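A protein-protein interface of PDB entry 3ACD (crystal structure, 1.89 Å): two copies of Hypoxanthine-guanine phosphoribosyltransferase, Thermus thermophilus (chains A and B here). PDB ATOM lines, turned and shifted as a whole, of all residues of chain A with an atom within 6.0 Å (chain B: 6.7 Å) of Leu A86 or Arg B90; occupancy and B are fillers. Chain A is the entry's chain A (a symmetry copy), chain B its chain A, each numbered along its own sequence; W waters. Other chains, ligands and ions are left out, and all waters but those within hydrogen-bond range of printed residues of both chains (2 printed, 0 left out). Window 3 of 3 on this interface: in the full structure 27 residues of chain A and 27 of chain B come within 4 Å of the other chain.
Among the printed residues, pairs that only touch across the chains: Asn A46 with Phe B67 (3.5 Å), Leu A86 with Lys B87 (3.9 Å), Leu A86 with Arg B90 (3.4 Å), Lys A87 with Lys B87 (2.8 Å) and Gln A165 with Leu B91 (3.7 Å).
Of chain B, only Lys B87 (3.9 Å) and Arg B90 (3.4 Å) come within 4 Å of Leu A86. Of chain A, only Leu A86 (3.4 Å) comes within 4 Å of Arg B90. Printed residues of chain A within 4 Å of Leu B91: Gln A165 (3.7 Å). Printed residues of chain B within 4 Å of Asn A46: Phe B67. Of the printed residues of chain B, Gln A165 touches Leu B91. Of the printed residues of chain A, Lys B87 touches Leu A86 (3.9 Å) and Lys A87 (2.8 Å). Printed residues of chain A within 4 Å of Phe B67: Asn A46 (3.5 Å). The nearest residue of chain B that does not touch Leu A86 is Asp B88 (6.6 Å). The nearest residue of chain A that does not touch Arg B90 is Asn A46 (4.3 Å).
Lys B87 touches its own counterpart, Lys A87. Of the 5 pairs that touch across the chains among the printed residues, 1 has its exchanged pair printed and touching as well.
Water W2 lies within hydrogen-bond range of the side-chain amide oxygen of Asn A46 (2.6 Å) and the side-chain carboxylate of Asp B66 (2.7 Å). Water W1 lies within hydrogen-bond range of the side-chain amide nitrogen of Gln A165 (3.0 Å) and the guanidinium group of Arg B90 (3.4 Å).
Hydrophobic or aromatic side chains of chain B within 4 Å of the printed part of chain A: Phe B67 and Leu B91. Of the 11 printed residues of chain A, 4 touch a printed residue of chain B. Printed residues of chain A that touch a printed residue of chain B: Asn A46, Leu A86, Lys A87 and Gln A165. Among the printed residues, 5 pairs touch across the chains. Among the printed residues, no Asp or Glu carboxylate lies within 4 Å of a Lys or Arg side-chain nitrogen of the other chain.
The backbone carbonyl oxygen (O) of Ala A69 lies within hydrogen-bond range of the backbone NH (N) of Leu A86 (2.6 Å). The side-chain carboxylate (OD2) of Asp B66 is in hydrogen-bond range of the backbone NH (N) of Leu B91, 3.0 Å away. The side-chain carboxylate of Asp B66 lies within hydrogen-bond range of the backbone NH of Arg B90. The backbone NH (N) of Lys A87 is in hydrogen-bond range of the backbone carbonyl oxygen (O) of Ala A69 (3.2 Å).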
ATOM      1  N   LEU A  45      31.912   4.326  27.937  1.00  0.00           N
ATOM      2  CA  LEU A  45      31.961   3.245  26.951  1.00  0.00           C
ATOM      3  C   LEU A  45      32.704   3.697  25.696  1.00  0.00           C
ATOM      4  O   LEU A  45      32.754   4.891  25.408  1.00  0.00           O
ATOM      5  CB  LEU A  45      30.535   2.820  26.579  1.00  0.00           C
ATOM      6  CG  LEU A  45      29.717   2.147  27.684  1.00  0.00           C
ATOM      7  CD1 LEU A  45      28.279   1.959  27.224  1.00  0.00           C
ATOM      8  CD2 LEU A  45      30.352   0.808  28.033  1.00  0.00           C
ATOM      9  N   ASN A  46      33.259   2.760  24.932  1.00  0.00           N
ATOM     10  CA  ASN A  46      33.196   1.323  25.212  1.00  0.00           C
ATOM     11  C   ASN A  46      34.412   0.815  25.985  1.00  0.00           C
ATOM     12  O   ASN A  46      34.324  -0.170  26.717  1.00  0.00           O
ATOM     13  CB  ASN A  46      33.135   0.530  23.897  1.00  0.00           C
ATOM     14  CG  ASN A  46      31.832   0.719  23.143  1.00  0.00           C
ATOM     15  OD1 ASN A  46      31.723   0.338  21.976  1.00  0.00           O
ATOM     16  ND2 ASN A  46      30.837   1.286  23.803  1.00  0.00           N
ATOM     17  N   ALA A  69      28.496   7.230  26.249  1.00  0.00           N
ATOM     18  CA  ALA A  69      29.397   7.072  25.114  1.00  0.00           C
ATOM     19  C   ALA A  69      29.791   8.462  24.639  1.00  0.00           C
ATOM     20  O   ALA A  69      28.933   9.318  24.425  1.00  0.00           O
ATOM     21  CB  ALA A  69      28.708   6.303  23.996  1.00  0.00           C
ATOM     22  N   ILE A  70      31.093   8.686  24.485  1.00  0.00           N
ATOM     23  CA  ILE A  70      31.605   9.978  24.046  1.00  0.00           C
ATOM     24  C   ILE A  70      32.666   9.778  22.964  1.00  0.00           C
ATOM     25  O   ILE A  70      33.245   8.698  22.844  1.00  0.00           O
ATOM     26  CB  ILE A  70      32.224  10.747  25.239  1.00  0.00           C
ATOM     27  CG1 ILE A  70      32.684  12.136  24.795  1.00  0.00           C
ATOM     28  CG2 ILE A  70      33.385   9.956  25.818  1.00  0.00           C
ATOM     29  CD1 ILE A  70      31.553  13.049  24.380  1.00  0.00           C
ATOM     30  N   SER A  71      32.913  10.820  22.174  1.00  0.00           N
ATOM     31  CA  SER A  71      33.906  10.751  21.108  1.00  0.00           C
ATOM     32  C   SER A  71      34.438  12.136  20.754  1.00  0.00           C
ATOM     33  O   SER A  71      33.713  13.129  20.830  1.00  0.00           O
ATOM     34  CB  SER A  71      33.297  10.098  19.865  1.00  0.00           C
ATOM     35  OG  SER A  71      32.843   8.788  20.152  1.00  0.00           O
ATOM     36  N   GLU A  84      31.162  15.021  20.726  1.00  0.00           N
ATOM     37  CA  GLU A  84      29.776  14.875  21.162  1.00  0.00           C
ATOM     38  C   GLU A  84      29.550  13.515  21.810  1.00  0.00           C
ATOM     39  O   GLU A  84      30.327  12.582  21.606  1.00  0.00           O
ATOM     40  CB  GLU A  84      28.831  15.042  19.970  1.00  0.00           C
ATOM     41  CG  GLU A  84      28.917  16.403  19.302  1.00  0.00           C
ATOM     42  CD  GLU A  84      28.593  17.540  20.251  1.00  0.00           C
ATOM     43  OE1 GLU A  84      27.464  17.570  20.782  1.00  0.00           O
ATOM     44  OE2 GLU A  84      29.471  18.402  20.466  1.00  0.00           O
ATOM     45  N   LEU A  85      28.481  13.406  22.595  1.00  0.00           N
ATOM     46  CA  LEU A  85      28.162  12.153  23.269  1.00  0.00           C
ATOM     47  C   LEU A  85      27.218  11.306  22.423  1.00  0.00           C
ATOM     48  O   LEU A  85      26.242  11.809  21.864  1.00  0.00           O
ATOM     49  CB  LEU A  85      27.530  12.424  24.640  1.00  0.00           C
ATOM     50  CG  LEU A  85      26.201  13.181  24.703  1.00  0.00           C
ATOM     51  CD1 LEU A  85      25.663  13.134  26.125  1.00  0.00           C
ATOM     52  CD2 LEU A  85      26.396  14.618  24.249  1.00  0.00           C
ATOM     53  N   LEU A  86      27.521  10.014  22.333  1.00  0.00           N
ATOM     54  CA  LEU A  86      26.714   9.084  21.553  1.00  0.00           C
ATOM     55  C   LEU A  86      25.710   8.352  22.441  1.00  0.00           C
ATOM     56  O   LEU A  86      24.820   7.658  21.948  1.00  0.00           O
ATOM     57  CB  LEU A  86      27.624   8.071  20.856  1.00  0.00           C
ATOM     58  CG  LEU A  86      28.804   8.660  20.074  1.00  0.00           C
ATOM     59  CD1 LEU A  86      29.602   7.536  19.430  1.00  0.00           C
ATOM     60  CD2 LEU A  86      28.299   9.629  19.016  1.00  0.00           C
ATOM     61  N   LYS A  87      25.864   8.514  23.753  1.00  0.00           N
ATOM     62  CA  LYS A  87      24.979   7.882  24.726  1.00  0.00           C
ATOM     63  C   LYS A  87      24.812   8.813  25.922  1.00  0.00           C
ATOM     64  O   LYS A  87      25.791   9.187  26.568  1.00  0.00           O
ATOM     65  CB  LYS A  87      25.567   6.545  25.189  1.00  0.00           C
ATOM     66  CG  LYS A  87      24.695   5.777  26.174  1.00  0.00           C
ATOM     67  CD  LYS A  87      23.377   5.355  25.544  1.00  0.00           C
ATOM     68  CE  LYS A  87      22.533   4.537  26.510  1.00  0.00           C
ATOM     69  NZ  LYS A  87      22.171   5.309  27.730  1.00  0.00           N
ATOM     70  N   ASP A  88      23.568   9.183  26.213  1.00  0.00           N
ATOM     71  CA  ASP A  88      23.279  10.085  27.323  1.00  0.00           C
ATOM     72  C   ASP A  88      23.104   9.374  28.660  1.00  0.00           C
ATOM     73  O   ASP A  88      22.943   8.155  28.718  1.00  0.00           O
ATOM     74  CB  ASP A  88      22.018  10.900  27.022  1.00  0.00           C
ATOM     75  CG  ASP A  88      22.176  11.789  25.808  1.00  0.00           C
ATOM     76  OD1 ASP A  88      22.447  11.258  24.712  1.00  0.00           O
ATOM     77  OD2 ASP A  88      22.028  13.021  25.953  1.00  0.00           O
ATOM     78  N   GLN A 165      38.532  -1.984  16.813  1.00  0.00           N
ATOM     79  CA  GLN A 165      37.396  -2.744  17.337  1.00  0.00           C
ATOM     80  C   GLN A 165      37.720  -4.146  17.860  1.00  0.00           C
ATOM     81  O   GLN A 165      36.906  -4.754  18.554  1.00  0.00           O
ATOM     82  CB  GLN A 165      36.286  -2.833  16.284  1.00  0.00           C
ATOM     83  CG  GLN A 165      35.647  -1.490  15.941  1.00  0.00           C
ATOM     84  CD  GLN A 165      35.094  -0.769  17.164  1.00  0.00           C
ATOM     85  OE1 GLN A 165      34.643  -1.398  18.125  1.00  0.00           O
ATOM     86  NE2 GLN A 165      35.115   0.557  17.126  1.00  0.00           N
ATOM     87  N   ASP B  66      29.746  -4.723  20.928  1.00  0.00           N
ATOM     88  CA  ASP B  66      28.880  -3.564  20.866  1.00  0.00           C
ATOM     89  C   ASP B  66      28.007  -3.616  22.116  1.00  0.00           C
ATOM     90  O   ASP B  66      27.936  -4.648  22.795  1.00  0.00           O
ATOM     91  CB  ASP B  66      28.016  -3.564  19.599  1.00  0.00           C
ATOM     92  CG  ASP B  66      27.673  -2.158  19.140  1.00  0.00           C
ATOM     93  OD1 ASP B  66      27.896  -1.211  19.925  1.00  0.00           O
ATOM     94  OD2 ASP B  66      27.181  -1.993  18.004  1.00  0.00           O
ATOM     95  N   PHE B  67      27.363  -2.498  22.424  1.00  0.00           N
ATOM     96  CA  PHE B  67      26.509  -2.398  23.598  1.00  0.00           C
ATOM     97  C   PHE B  67      25.170  -1.792  23.208  1.00  0.00           C
ATOM     98  O   PHE B  67      25.113  -0.862  22.402  1.00  0.00           O
ATOM     99  CB  PHE B  67      27.187  -1.522  24.655  1.00  0.00           C
ATOM    100  CG  PHE B  67      28.462  -2.103  25.192  1.00  0.00           C
ATOM    101  CD1 PHE B  67      28.463  -2.833  26.377  1.00  0.00           C
ATOM    102  CD2 PHE B  67      29.655  -1.961  24.492  1.00  0.00           C
ATOM    103  CE1 PHE B  67      29.634  -3.415  26.858  1.00  0.00           C
ATOM    104  CE2 PHE B  67      30.833  -2.540  24.964  1.00  0.00           C
ATOM    105  CZ  PHE B  67      30.821  -3.269  26.147  1.00  0.00           C
ATOM    106  N   ILE B  68      24.096  -2.329  23.772  1.00  0.00           N
ATOM    107  CA  ILE B  68      22.759  -1.826  23.489  1.00  0.00           C
ATOM    108  C   ILE B  68      21.938  -1.782  24.772  1.00  0.00           C
ATOM    109  O   ILE B  68      22.169  -2.561  25.693  1.00  0.00           O
ATOM    110  CB  ILE B  68      22.026  -2.726  22.477  1.00  0.00           C
ATOM    111  CG1 ILE B  68      21.915  -4.146  23.035  1.00  0.00           C
ATOM    112  CG2 ILE B  68      22.759  -2.718  21.150  1.00  0.00           C
ATOM    113  CD1 ILE B  68      21.159  -5.099  22.146  1.00  0.00           C
ATOM    114  N   LYS B  87      19.422   2.412  23.544  1.00  0.00           N
ATOM    115  CA  LYS B  87      20.762   2.551  22.980  1.00  0.00           C
ATOM    116  C   LYS B  87      20.862   1.693  21.723  1.00  0.00           C
ATOM    117  O   LYS B  87      20.655   0.481  21.774  1.00  0.00           O
ATOM    118  CB  LYS B  87      21.816   2.104  23.998  1.00  0.00           C
ATOM    119  CG  LYS B  87      23.255   2.254  23.525  1.00  0.00           C
ATOM    120  CD  LYS B  87      23.620   3.712  23.295  1.00  0.00           C
ATOM    121  CE  LYS B  87      25.076   3.865  22.881  1.00  0.00           C
ATOM    122  NZ  LYS B  87      25.371   3.167  21.599  1.00  0.00           N
ATOM    123  N   ASP B  88      21.180   2.327  20.599  1.00  0.00           N
ATOM    124  CA  ASP B  88      21.291   1.621  19.327  1.00  0.00           C
ATOM    125  C   ASP B  88      22.670   1.022  19.077  1.00  0.00           C
ATOM    126  O   ASP B  88      23.643   1.359  19.751  1.00  0.00           O
ATOM    127  CB  ASP B  88      20.936   2.561  18.173  1.00  0.00           C
ATOM    128  CG  ASP B  88      19.507   3.052  18.240  1.00  0.00           C
ATOM    129  OD1 ASP B  88      19.142   3.685  19.251  1.00  0.00           O
ATOM    130  OD2 ASP B  88      18.749   2.804  17.279  1.00  0.00           O
ATOM    131  N   LEU B  89      22.731   0.134  18.089  1.00  0.00           N
ATOM    132  CA  LEU B  89      23.967  -0.532  17.699  1.00  0.00           C
ATOM    133  C   LEU B  89      24.833   0.435  16.898  1.00  0.00           C
ATOM    134  O   LEU B  89      24.313   1.289  16.181  1.00  0.00           O
ATOM    135  CB  LEU B  89      23.655  -1.764  16.839  1.00  0.00           C
ATOM    136  CG  LEU B  89      22.893  -2.948  17.449  1.00  0.00           C
ATOM    137  CD1 LEU B  89      21.547  -2.500  17.997  1.00  0.00           C
ATOM    138  CD2 LEU B  89      22.693  -4.011  16.382  1.00  0.00           C
ATOM    139  N   ARG B  90      26.150   0.294  17.018  1.00  0.00           N
ATOM    140  CA  ARG B  90      27.084   1.156  16.302  1.00  0.00           C
ATOM    141  C   ARG B  90      27.829   0.410  15.200  1.00  0.00           C
ATOM    142  O   ARG B  90      28.188   0.998  14.179  1.00  0.00           O
ATOM    143  CB  ARG B  90      28.091   1.770  17.278  1.00  0.00           C
ATOM    144  CG  ARG B  90      27.492   2.788  18.231  1.00  0.00           C
ATOM    145  CD  ARG B  90      28.513   3.257  19.254  1.00  0.00           C
ATOM    146  NE  ARG B  90      29.709   3.811  18.624  1.00  0.00           N
ATOM    147  CZ  ARG B  90      30.754   4.288  19.294  1.00  0.00           C
ATOM    148  NH1 ARG B  90      30.758   4.282  20.621  1.00  0.00           N
ATOM    149  NH2 ARG B  90      31.800   4.772  18.636  1.00  0.00           N
ATOM    150  N   LEU B  91      28.065  -0.880  15.410  1.00  0.00           N
ATOM    151  CA  LEU B  91      28.769  -1.702  14.432  1.00  0.00           C
ATOM    152  C   LEU B  91      27.782  -2.535  13.623  1.00  0.00           C
ATOM    153  O   LEU B  91      26.724  -2.915  14.116  1.00  0.00           O
ATOM    154  CB  LEU B  91      29.775  -2.622  15.131  1.00  0.00           C
ATOM    155  CG  LEU B  91      31.066  -1.981  15.658  1.00  0.00           C
ATOM    156  CD1 LEU B  91      30.749  -0.906  16.684  1.00  0.00           C
ATOM    157  CD2 LEU B  91      31.943  -3.056  16.273  1.00  0.00           C
ATOM    158  N   PRO B  92      28.116  -2.822  12.356  1.00  0.00           N
ATOM    159  CA  PRO B  92      27.237  -3.614  11.491  1.00  0.00           C
ATOM    160  C   PRO B  92      27.095  -5.049  11.984  1.00  0.00           C
ATOM    161  O   PRO B  92      28.048  -5.625  12.507  1.00  0.00           O
ATOM    162  CB  PRO B  92      27.940  -3.557  10.133  1.00  0.00           C
ATOM    163  CG  PRO B  92      28.723  -2.274  10.191  1.00  0.00           C
ATOM    164  CD  PRO B  92      29.267  -2.302  11.598  1.00  0.00           C
ATOM    165  N   ARG B 121      18.236  -7.501  10.428  1.00  0.00           N
ATOM    166  CA  ARG B 121      19.407  -6.997   9.716  1.00  0.00           C
ATOM    167  C   ARG B 121      20.171  -8.110   9.013  1.00  0.00           C
ATOM    168  O   ARG B 121      21.216  -7.879   8.405  1.00  0.00           O
ATOM    169  CB  ARG B 121      20.327  -6.238  10.669  1.00  0.00           C
ATOM    170  CG  ARG B 121      19.696  -4.964  11.195  1.00  0.00           C
ATOM    171  CD  ARG B 121      20.738  -4.042  11.771  1.00  0.00           C
ATOM    172  NE  ARG B 121      20.160  -2.768  12.183  1.00  0.00           N
ATOM    173  CZ  ARG B 121      20.877  -1.711  12.539  1.00  0.00           C
ATOM    174  NH1 ARG B 121      22.198  -1.778  12.530  1.00  0.00           N
ATOM    175  NH2 ARG B 121      20.271  -0.593  12.910  1.00  0.00           N
HETATM  176  O   HOH W   1      33.741   2.038  19.320  1.00  0.00           O
HETATM  177  O   HOH W   2      29.980   0.497  20.032  1.00  0.00           O
